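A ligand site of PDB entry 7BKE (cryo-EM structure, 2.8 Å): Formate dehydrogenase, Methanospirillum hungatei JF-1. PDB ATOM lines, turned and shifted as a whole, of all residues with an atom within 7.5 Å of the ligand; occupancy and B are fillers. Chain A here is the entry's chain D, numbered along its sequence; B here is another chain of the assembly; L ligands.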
ATOM      1  N   THR A  14      12.006  12.691  30.322  1.00  0.00           N
ATOM      2  CA  THR A  14      12.130  13.723  29.304  1.00  0.00           C
ATOM      3  C   THR A  14      13.593  13.880  28.890  1.00  0.00           C
ATOM      4  O   THR A  14      14.499  13.737  29.706  1.00  0.00           O
ATOM      5  CB  THR A  14      11.593  15.049  29.837  1.00  0.00           C
ATOM      6  OG1 THR A  14      10.301  14.829  30.389  1.00  0.00           O
ATOM      7  CG2 THR A  14      11.490  16.067  28.750  1.00  0.00           C
ATOM      8  N   CYS A  15      13.797  14.177  27.619  1.00  0.00           N
ATOM      9  CA  CYS A  15      15.151  14.424  27.139  1.00  0.00           C
ATOM     10  C   CYS A  15      15.665  15.740  27.705  1.00  0.00           C
ATOM     11  O   CYS A  15      14.928  16.736  27.721  1.00  0.00           O
ATOM     12  CB  CYS A  15      15.178  14.459  25.620  1.00  0.00           C
ATOM     13  SG  CYS A  15      16.801  14.751  24.902  1.00  0.00           S
ATOM     14  N   PRO A  16      16.895  15.790  28.194  1.00  0.00           N
ATOM     15  CA  PRO A  16      17.387  17.019  28.824  1.00  0.00           C
ATOM     16  C   PRO A  16      18.138  17.965  27.903  1.00  0.00           C
ATOM     17  O   PRO A  16      18.832  18.845  28.396  1.00  0.00           O
ATOM     18  CB  PRO A  16      18.337  16.474  29.888  1.00  0.00           C
ATOM     19  CG  PRO A  16      18.874  15.258  29.288  1.00  0.00           C
ATOM     20  CD  PRO A  16      17.808  14.665  28.422  1.00  0.00           C
ATOM     21  N   TYR A  17      18.043  17.807  26.588  1.00  0.00           N
ATOM     22  CA  TYR A  17      18.979  18.493  25.717  1.00  0.00           C
ATOM     23  C   TYR A  17      18.439  19.691  24.983  1.00  0.00           C
ATOM     24  O   TYR A  17      19.243  20.507  24.517  1.00  0.00           O
ATOM     25  CB  TYR A  17      19.567  17.516  24.704  1.00  0.00           C
ATOM     26  CG  TYR A  17      20.619  16.656  25.335  1.00  0.00           C
ATOM     27  CD1 TYR A  17      20.597  15.295  25.209  1.00  0.00           C
ATOM     28  CD2 TYR A  17      21.620  17.234  26.077  1.00  0.00           C
ATOM     29  CE1 TYR A  17      21.554  14.519  25.790  1.00  0.00           C
ATOM     30  CE2 TYR A  17      22.581  16.472  26.667  1.00  0.00           C
ATOM     31  CZ  TYR A  17      22.545  15.118  26.525  1.00  0.00           C
ATOM     32  OH  TYR A  17      23.500  14.349  27.117  1.00  0.00           O
ATOM     33  N   CYS A  18      17.132  19.857  24.844  1.00  0.00           N
ATOM     34  CA  CYS A  18      16.600  21.115  24.332  1.00  0.00           C
ATOM     35  C   CYS A  18      15.159  21.250  24.785  1.00  0.00           C
ATOM     36  O   CYS A  18      14.638  20.418  25.526  1.00  0.00           O
ATOM     37  CB  CYS A  18      16.739  21.212  22.810  1.00  0.00           C
ATOM     38  SG  CYS A  18      15.558  20.311  21.845  1.00  0.00           S
ATOM     39  N   GLY A  19      14.521  22.314  24.341  1.00  0.00           N
ATOM     40  CA  GLY A  19      13.225  22.709  24.828  1.00  0.00           C
ATOM     41  C   GLY A  19      12.040  22.011  24.227  1.00  0.00           C
ATOM     42  O   GLY A  19      10.908  22.337  24.585  1.00  0.00           O
ATOM     43  N   VAL A  20      12.242  21.054  23.314  1.00  0.00           N
ATOM     44  CA  VAL A  20      11.122  20.311  22.774  1.00  0.00           C
ATOM     45  C   VAL A  20      10.515  19.419  23.851  1.00  0.00           C
ATOM     46  O   VAL A  20       9.293  19.248  23.933  1.00  0.00           O
ATOM     47  CB  VAL A  20      11.548  19.506  21.543  1.00  0.00           C
ATOM     48  CG1 VAL A  20      10.377  18.753  20.991  1.00  0.00           C
ATOM     49  CG2 VAL A  20      12.090  20.420  20.490  1.00  0.00           C
ATOM     50  N   GLY A  21      11.347  18.843  24.704  1.00  0.00           N
ATOM     51  CA  GLY A  21      10.838  18.006  25.763  1.00  0.00           C
ATOM     52  C   GLY A  21      10.396  16.641  25.331  1.00  0.00           C
ATOM     53  O   GLY A  21       9.390  16.140  25.828  1.00  0.00           O
ATOM     54  N   CYS A  22      11.135  16.012  24.424  1.00  0.00           N
ATOM     55  CA  CYS A  22      10.755  14.697  23.944  1.00  0.00           C
ATOM     56  C   CYS A  22      10.794  13.693  25.078  1.00  0.00           C
ATOM     57  O   CYS A  22      11.556  13.830  26.021  1.00  0.00           O
ATOM     58  CB  CYS A  22      11.687  14.269  22.816  1.00  0.00           C
ATOM     59  SG  CYS A  22      11.729  15.396  21.432  1.00  0.00           S
ATOM     60  N   THR A  23       9.953  12.674  24.981  1.00  0.00           N
ATOM     61  CA  THR A  23       9.893  11.620  25.973  1.00  0.00           C
ATOM     62  C   THR A  23      10.640  10.400  25.462  1.00  0.00           C
ATOM     63  O   THR A  23      10.606  10.095  24.276  1.00  0.00           O
ATOM     64  CB  THR A  23       8.449  11.251  26.276  1.00  0.00           C
ATOM     65  OG1 THR A  23       7.707  12.444  26.538  1.00  0.00           O
ATOM     66  CG2 THR A  23       8.370  10.366  27.488  1.00  0.00           C
ATOM     67  N   LEU A  24      11.326   9.719  26.376  1.00  0.00           N
ATOM     68  CA  LEU A  24      12.114   8.567  26.008  1.00  0.00           C
ATOM     69  C   LEU A  24      12.114   7.602  27.168  1.00  0.00           C
ATOM     70  O   LEU A  24      11.796   7.961  28.300  1.00  0.00           O
ATOM     71  CB  LEU A  24      13.535   8.983  25.617  1.00  0.00           C
ATOM     72  CG  LEU A  24      14.384   9.770  26.620  1.00  0.00           C
ATOM     73  CD1 LEU A  24      15.142   8.856  27.541  1.00  0.00           C
ATOM     74  CD2 LEU A  24      15.323  10.676  25.894  1.00  0.00           C
ATOM     75  N   ILE A  44       4.326  14.561  22.192  1.00  0.00           N
ATOM     76  CA  ILE A  44       5.325  15.544  21.678  1.00  0.00           C
ATOM     77  C   ILE A  44       6.138  14.976  20.536  1.00  0.00           C
ATOM     78  O   ILE A  44       6.246  15.633  19.511  1.00  0.00           O
ATOM     79  CB  ILE A  44       6.272  15.933  22.833  1.00  0.00           C
ATOM     80  CG1 ILE A  44       5.499  16.459  24.046  1.00  0.00           C
ATOM     81  CG2 ILE A  44       7.337  16.914  22.368  1.00  0.00           C
ATOM     82  CD1 ILE A  44       5.904  15.825  25.339  1.00  0.00           C
ATOM     83  N   ASN A  45       6.666  13.786  20.715  1.00  0.00           N
ATOM     84  CA  ASN A  45       7.483  13.090  19.713  1.00  0.00           C
ATOM     85  C   ASN A  45       6.819  11.738  19.757  1.00  0.00           C
ATOM     86  O   ASN A  45       6.483  11.307  20.825  1.00  0.00           O
ATOM     87  CB  ASN A  45       8.884  12.939  20.277  1.00  0.00           C
ATOM     88  CG  ASN A  45       9.020  12.162  21.562  1.00  0.00           C
ATOM     89  OD1 ASN A  45       8.314  12.422  22.528  1.00  0.00           O
ATOM     90  ND2 ASN A  45       9.931  11.220  21.605  1.00  0.00           N
ATOM     91  N   LYS A  48      10.015   9.297  18.519  1.00  0.00           N
ATOM     92  CA  LYS A  48      11.082   9.708  17.601  1.00  0.00           C
ATOM     93  C   LYS A  48      12.009  10.605  18.388  1.00  0.00           C
ATOM     94  O   LYS A  48      11.530  11.296  19.244  1.00  0.00           O
ATOM     95  CB  LYS A  48      10.451  10.377  16.386  1.00  0.00           C
ATOM     96  CG  LYS A  48       9.337   9.593  15.736  1.00  0.00           C
ATOM     97  CD  LYS A  48       8.485  10.438  14.843  1.00  0.00           C
ATOM     98  CE  LYS A  48       7.459   9.621  14.094  1.00  0.00           C
ATOM     99  NZ  LYS A  48       7.910   9.318  12.725  1.00  0.00           N
ATOM    100  N   LEU A  49      13.309  10.466  18.195  1.00  0.00           N
ATOM    101  CA  LEU A  49      14.298  11.238  18.959  1.00  0.00           C
ATOM    102  C   LEU A  49      15.390  11.622  17.978  1.00  0.00           C
ATOM    103  O   LEU A  49      15.503  10.931  16.988  1.00  0.00           O
ATOM    104  CB  LEU A  49      14.867  10.377  20.084  1.00  0.00           C
ATOM    105  CG  LEU A  49      13.929   9.966  21.209  1.00  0.00           C
ATOM    106  CD1 LEU A  49      14.448   8.725  21.898  1.00  0.00           C
ATOM    107  CD2 LEU A  49      13.781  11.094  22.215  1.00  0.00           C
ATOM    108  N   CYS A  50      16.115  12.694  18.250  1.00  0.00           N
ATOM    109  CA  CYS A  50      17.224  13.171  17.443  1.00  0.00           C
ATOM    110  C   CYS A  50      18.487  12.471  17.911  1.00  0.00           C
ATOM    111  O   CYS A  50      18.418  11.642  18.827  1.00  0.00           O
ATOM    112  CB  CYS A  50      17.346  14.687  17.570  1.00  0.00           C
ATOM    113  SG  CYS A  50      18.074  15.288  19.065  1.00  0.00           S
ATOM    114  N   PRO A  51      19.656  12.727  17.311  1.00  0.00           N
ATOM    115  CA  PRO A  51      20.874  12.075  17.807  1.00  0.00           C
ATOM    116  C   PRO A  51      21.145  12.312  19.277  1.00  0.00           C
ATOM    117  O   PRO A  51      21.577  11.399  19.995  1.00  0.00           O
ATOM    118  CB  PRO A  51      21.967  12.677  16.929  1.00  0.00           C
ATOM    119  CG  PRO A  51      21.292  13.044  15.694  1.00  0.00           C
ATOM    120  CD  PRO A  51      19.891  13.381  16.009  1.00  0.00           C
ATOM    121  N   LYS A  52      20.905  13.534  19.758  1.00  0.00           N
ATOM    122  CA  LYS A  52      21.162  13.847  21.157  1.00  0.00           C
ATOM    123  C   LYS A  52      20.273  13.018  22.066  1.00  0.00           C
ATOM    124  O   LYS A  52      20.734  12.494  23.087  1.00  0.00           O
ATOM    125  CB  LYS A  52      20.951  15.331  21.396  1.00  0.00           C
ATOM    126  CG  LYS A  52      21.913  16.177  20.629  1.00  0.00           C
ATOM    127  CD  LYS A  52      21.929  17.601  21.145  1.00  0.00           C
ATOM    128  CE  LYS A  52      20.837  18.428  20.520  1.00  0.00           C
ATOM    129  NZ  LYS A  52      20.958  19.864  20.874  1.00  0.00           N
ATOM    130  N   GLY A  53      18.993  12.895  21.739  1.00  0.00           N
ATOM    131  CA  GLY A  53      18.119  12.058  22.534  1.00  0.00           C
ATOM    132  C   GLY A  53      18.485  10.598  22.449  1.00  0.00           C
ATOM    133  O   GLY A  53      18.387   9.867  23.439  1.00  0.00           O
ATOM    134  N   VAL A  54      18.918  10.144  21.284  1.00  0.00           N
ATOM    135  CA  VAL A  54      19.270   8.745  21.128  1.00  0.00           C
ATOM    136  C   VAL A  54      20.467   8.390  21.981  1.00  0.00           C
ATOM    137  O   VAL A  54      20.556   7.273  22.517  1.00  0.00           O
ATOM    138  CB  VAL A  54      19.504   8.425  19.641  1.00  0.00           C
ATOM    139  CG1 VAL A  54      20.229   7.132  19.495  1.00  0.00           C
ATOM    140  CG2 VAL A  54      18.192   8.341  18.916  1.00  0.00           C
ATOM    141  N   CYS A  56      21.577  10.240  24.765  1.00  0.00           N
ATOM    142  CA  CYS A  56      21.589  10.929  26.050  1.00  0.00           C
ATOM    143  C   CYS A  56      22.061  10.063  27.203  1.00  0.00           C
ATOM    144  O   CYS A  56      22.424  10.599  28.254  1.00  0.00           O
ATOM    145  CB  CYS A  56      20.195  11.465  26.370  1.00  0.00           C
ATOM    146  SG  CYS A  56      18.946  10.205  26.633  1.00  0.00           S
ATOM    147  N   GLU A 180      18.316  21.834  12.770  1.00  0.00           N
ATOM    148  CA  GLU A 180      19.572  21.608  13.468  1.00  0.00           C
ATOM    149  C   GLU A 180      19.368  21.636  14.970  1.00  0.00           C
ATOM    150  O   GLU A 180      19.795  20.730  15.690  1.00  0.00           O
ATOM    151  CB  GLU A 180      20.606  22.643  13.047  1.00  0.00           C
ATOM    152  CG  GLU A 180      21.160  22.444  11.645  1.00  0.00           C
ATOM    153  CD  GLU A 180      20.427  23.258  10.597  1.00  0.00           C
ATOM    154  OE1 GLU A 180      19.306  23.721  10.874  1.00  0.00           O
ATOM    155  OE2 GLU A 180      20.993  23.435   9.496  1.00  0.00           O
ATOM    156  N   ALA A 181      18.720  22.677  15.467  1.00  0.00           N
ATOM    157  CA  ALA A 181      18.310  22.771  16.856  1.00  0.00           C
ATOM    158  C   ALA A 181      16.796  22.643  16.902  1.00  0.00           C
ATOM    159  O   ALA A 181      16.099  23.260  16.091  1.00  0.00           O
ATOM    160  CB  ALA A 181      18.747  24.104  17.474  1.00  0.00           C
ATOM    161  N   HIS A 182      16.298  21.840  17.827  1.00  0.00           N
ATOM    162  CA  HIS A 182      14.899  21.428  17.908  1.00  0.00           C
ATOM    163  C   HIS A 182      14.460  20.591  16.700  1.00  0.00           C
ATOM    164  O   HIS A 182      13.428  20.903  16.082  1.00  0.00           O
ATOM    165  CB  HIS A 182      13.983  22.641  18.034  1.00  0.00           C
ATOM    166  CG  HIS A 182      14.566  23.739  18.868  1.00  0.00           C
ATOM    167  ND1 HIS A 182      15.291  24.777  18.322  1.00  0.00           N
ATOM    168  CD2 HIS A 182      14.527  23.972  20.193  1.00  0.00           C
ATOM    169  CE1 HIS A 182      15.676  25.591  19.284  1.00  0.00           C
ATOM    170  NE2 HIS A 182      15.223  25.123  20.432  1.00  0.00           N
ATOM    171  N   PRO A 183      15.170  19.525  16.362  1.00  0.00           N
ATOM    172  CA  PRO A 183      14.758  18.724  15.196  1.00  0.00           C
ATOM    173  C   PRO A 183      13.356  18.177  15.281  1.00  0.00           C
ATOM    174  O   PRO A 183      12.701  18.034  14.242  1.00  0.00           O
ATOM    175  CB  PRO A 183      15.789  17.599  15.162  1.00  0.00           C
ATOM    176  CG  PRO A 183      16.569  17.727  16.367  1.00  0.00           C
ATOM    177  CD  PRO A 183      16.482  19.093  16.849  1.00  0.00           C
ATOM    178  N   LEU A 184      12.840  17.872  16.462  1.00  0.00           N
ATOM    179  CA  LEU A 184      11.474  17.377  16.510  1.00  0.00           C
ATOM    180  C   LEU A 184      10.465  18.493  16.675  1.00  0.00           C
ATOM    181  O   LEU A 184       9.269  18.215  16.791  1.00  0.00           O
ATOM    182  CB  LEU A 184      11.311  16.330  17.607  1.00  0.00           C
ATOM    183  CG  LEU A 184      11.828  14.993  17.104  1.00  0.00           C
ATOM    184  CD1 LEU A 184      13.324  14.908  17.026  1.00  0.00           C
ATOM    185  CD2 LEU A 184      11.317  13.896  17.932  1.00  0.00           C
ATOM    186  N   ALA A 185      10.902  19.745  16.681  1.00  0.00           N
ATOM    187  CA  ALA A 185      10.012  20.833  16.326  1.00  0.00           C
ATOM    188  C   ALA A 185       9.982  21.029  14.816  1.00  0.00           C
ATOM    189  O   ALA A 185       8.931  21.324  14.249  1.00  0.00           O
ATOM    190  CB  ALA A 185      10.425  22.122  17.030  1.00  0.00           C
ATOM    191  N   GLY A 333      15.716  26.549  23.287  1.00  0.00           N
ATOM    192  CA  GLY A 333      17.044  26.003  23.091  1.00  0.00           C
ATOM    193  C   GLY A 333      17.618  25.236  24.266  1.00  0.00           C
ATOM    194  O   GLY A 333      18.457  24.351  24.056  1.00  0.00           O
ATOM    195  N   ASN A 335      16.820  22.909  27.870  1.00  0.00           N
ATOM    196  CA  ASN A 335      15.744  21.973  28.199  1.00  0.00           C
ATOM    197  C   ASN A 335      14.769  22.546  29.201  1.00  0.00           C
ATOM    198  O   ASN A 335      13.575  22.245  29.134  1.00  0.00           O
ATOM    199  CB  ASN A 335      16.301  20.656  28.713  1.00  0.00           C
ATOM    200  CG  ASN A 335      16.940  20.788  30.060  1.00  0.00           C
ATOM    201  OD1 ASN A 335      17.103  21.887  30.566  1.00  0.00           O
ATOM    202  ND2 ASN A 335      17.271  19.671  30.671  1.00  0.00           N
ATOM    203  N   ILE B 294      18.376  13.527   9.095  1.00  0.00           N
ATOM    204  CA  ILE B 294      19.268  14.221   9.997  1.00  0.00           C
ATOM    205  C   ILE B 294      20.267  13.274  10.650  1.00  0.00           C
ATOM    206  O   ILE B 294      20.936  13.661  11.604  1.00  0.00           O
ATOM    207  CB  ILE B 294      18.496  14.995  11.075  1.00  0.00           C
ATOM    208  CG1 ILE B 294      17.502  14.078  11.780  1.00  0.00           C
ATOM    209  CG2 ILE B 294      17.787  16.170  10.463  1.00  0.00           C
ATOM    210  CD1 ILE B 294      17.150  14.523  13.150  1.00  0.00           C
HETATM  211 FE1  LIG L   1      16.219  15.903  23.056  1.00  0.00          FE
HETATM  212 FE2  LIG L   1      13.924  15.866  21.592  1.00  0.00          FE
HETATM  213 FE3  LIG L   1      16.339  15.892  20.338  1.00  0.00          FE
HETATM  214 FE4  LIG L   1      15.456  18.114  21.648  1.00  0.00          FE
HETATM  215  S1  LIG L   1      14.523  17.150  19.821  1.00  0.00           S
HETATM  216  S2  LIG L   1      17.540  17.212  21.750  1.00  0.00           S
HETATM  217  S3  LIG L   1      14.361  17.165  23.395  1.00  0.00           S
HETATM  218  S4  LIG L   1      15.514  14.248  21.668  1.00  0.00           S
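FE4 of the ligand is bound by SG of Cys 18 (2.2 Å). SG of Cys 50 is bound to FE3 of the ligand (2.2 Å). N of Cys 22 sits close to S3 of the ligand, at 3.6 Å. The side-chain sulfur (SG) of Cys 22 is bound to an iron atom (FE2) of the ligand, 2.3 Å away. FE1 of the ligand is bound by SG of Cys 15, 2.3 Å away. N of Gly 53 lies close to S4 of the ligand. A sulfur (S3) of the ligand sits close to the backbone NH of Gly 21 (3.7 Å).
SG of Cys 18 lies close to N of Val 20 (3.7 Å). The side-chain sulfur of Cys 50 lies close to the backbone NH of Gly 53 (3.7 Å). SG of Cys 50 lies close to N of Lys 52, 3.4 Å away. O of Cys 22 sits at hydrogen-bond distance from N of Cys 15. The side-chain sulfur (SG) of Cys 15 sits close to the backbone NH (N) of Tyr 17 (3.7 Å). The side-chain sulfur (SG) of Cys 56 sits at hydrogen-bond distance from the backbone carbonyl oxygen (O) of Gly 53, 3.3 Å away.
Tyr 17 touches the ligand. Leu 49 touches the ligand (CD2 to S4, 3.6 Å). Lys 52 touches the ligand (CE to S2, 3.7 Å). Leu 184 touches the ligand. Hydrophobic or aromatic side chains within 4 Å of the ligand: Tyr 17, Leu 49 and Leu 184. Of the 30 residues printed, 10 come within 4 Å of the ligand.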
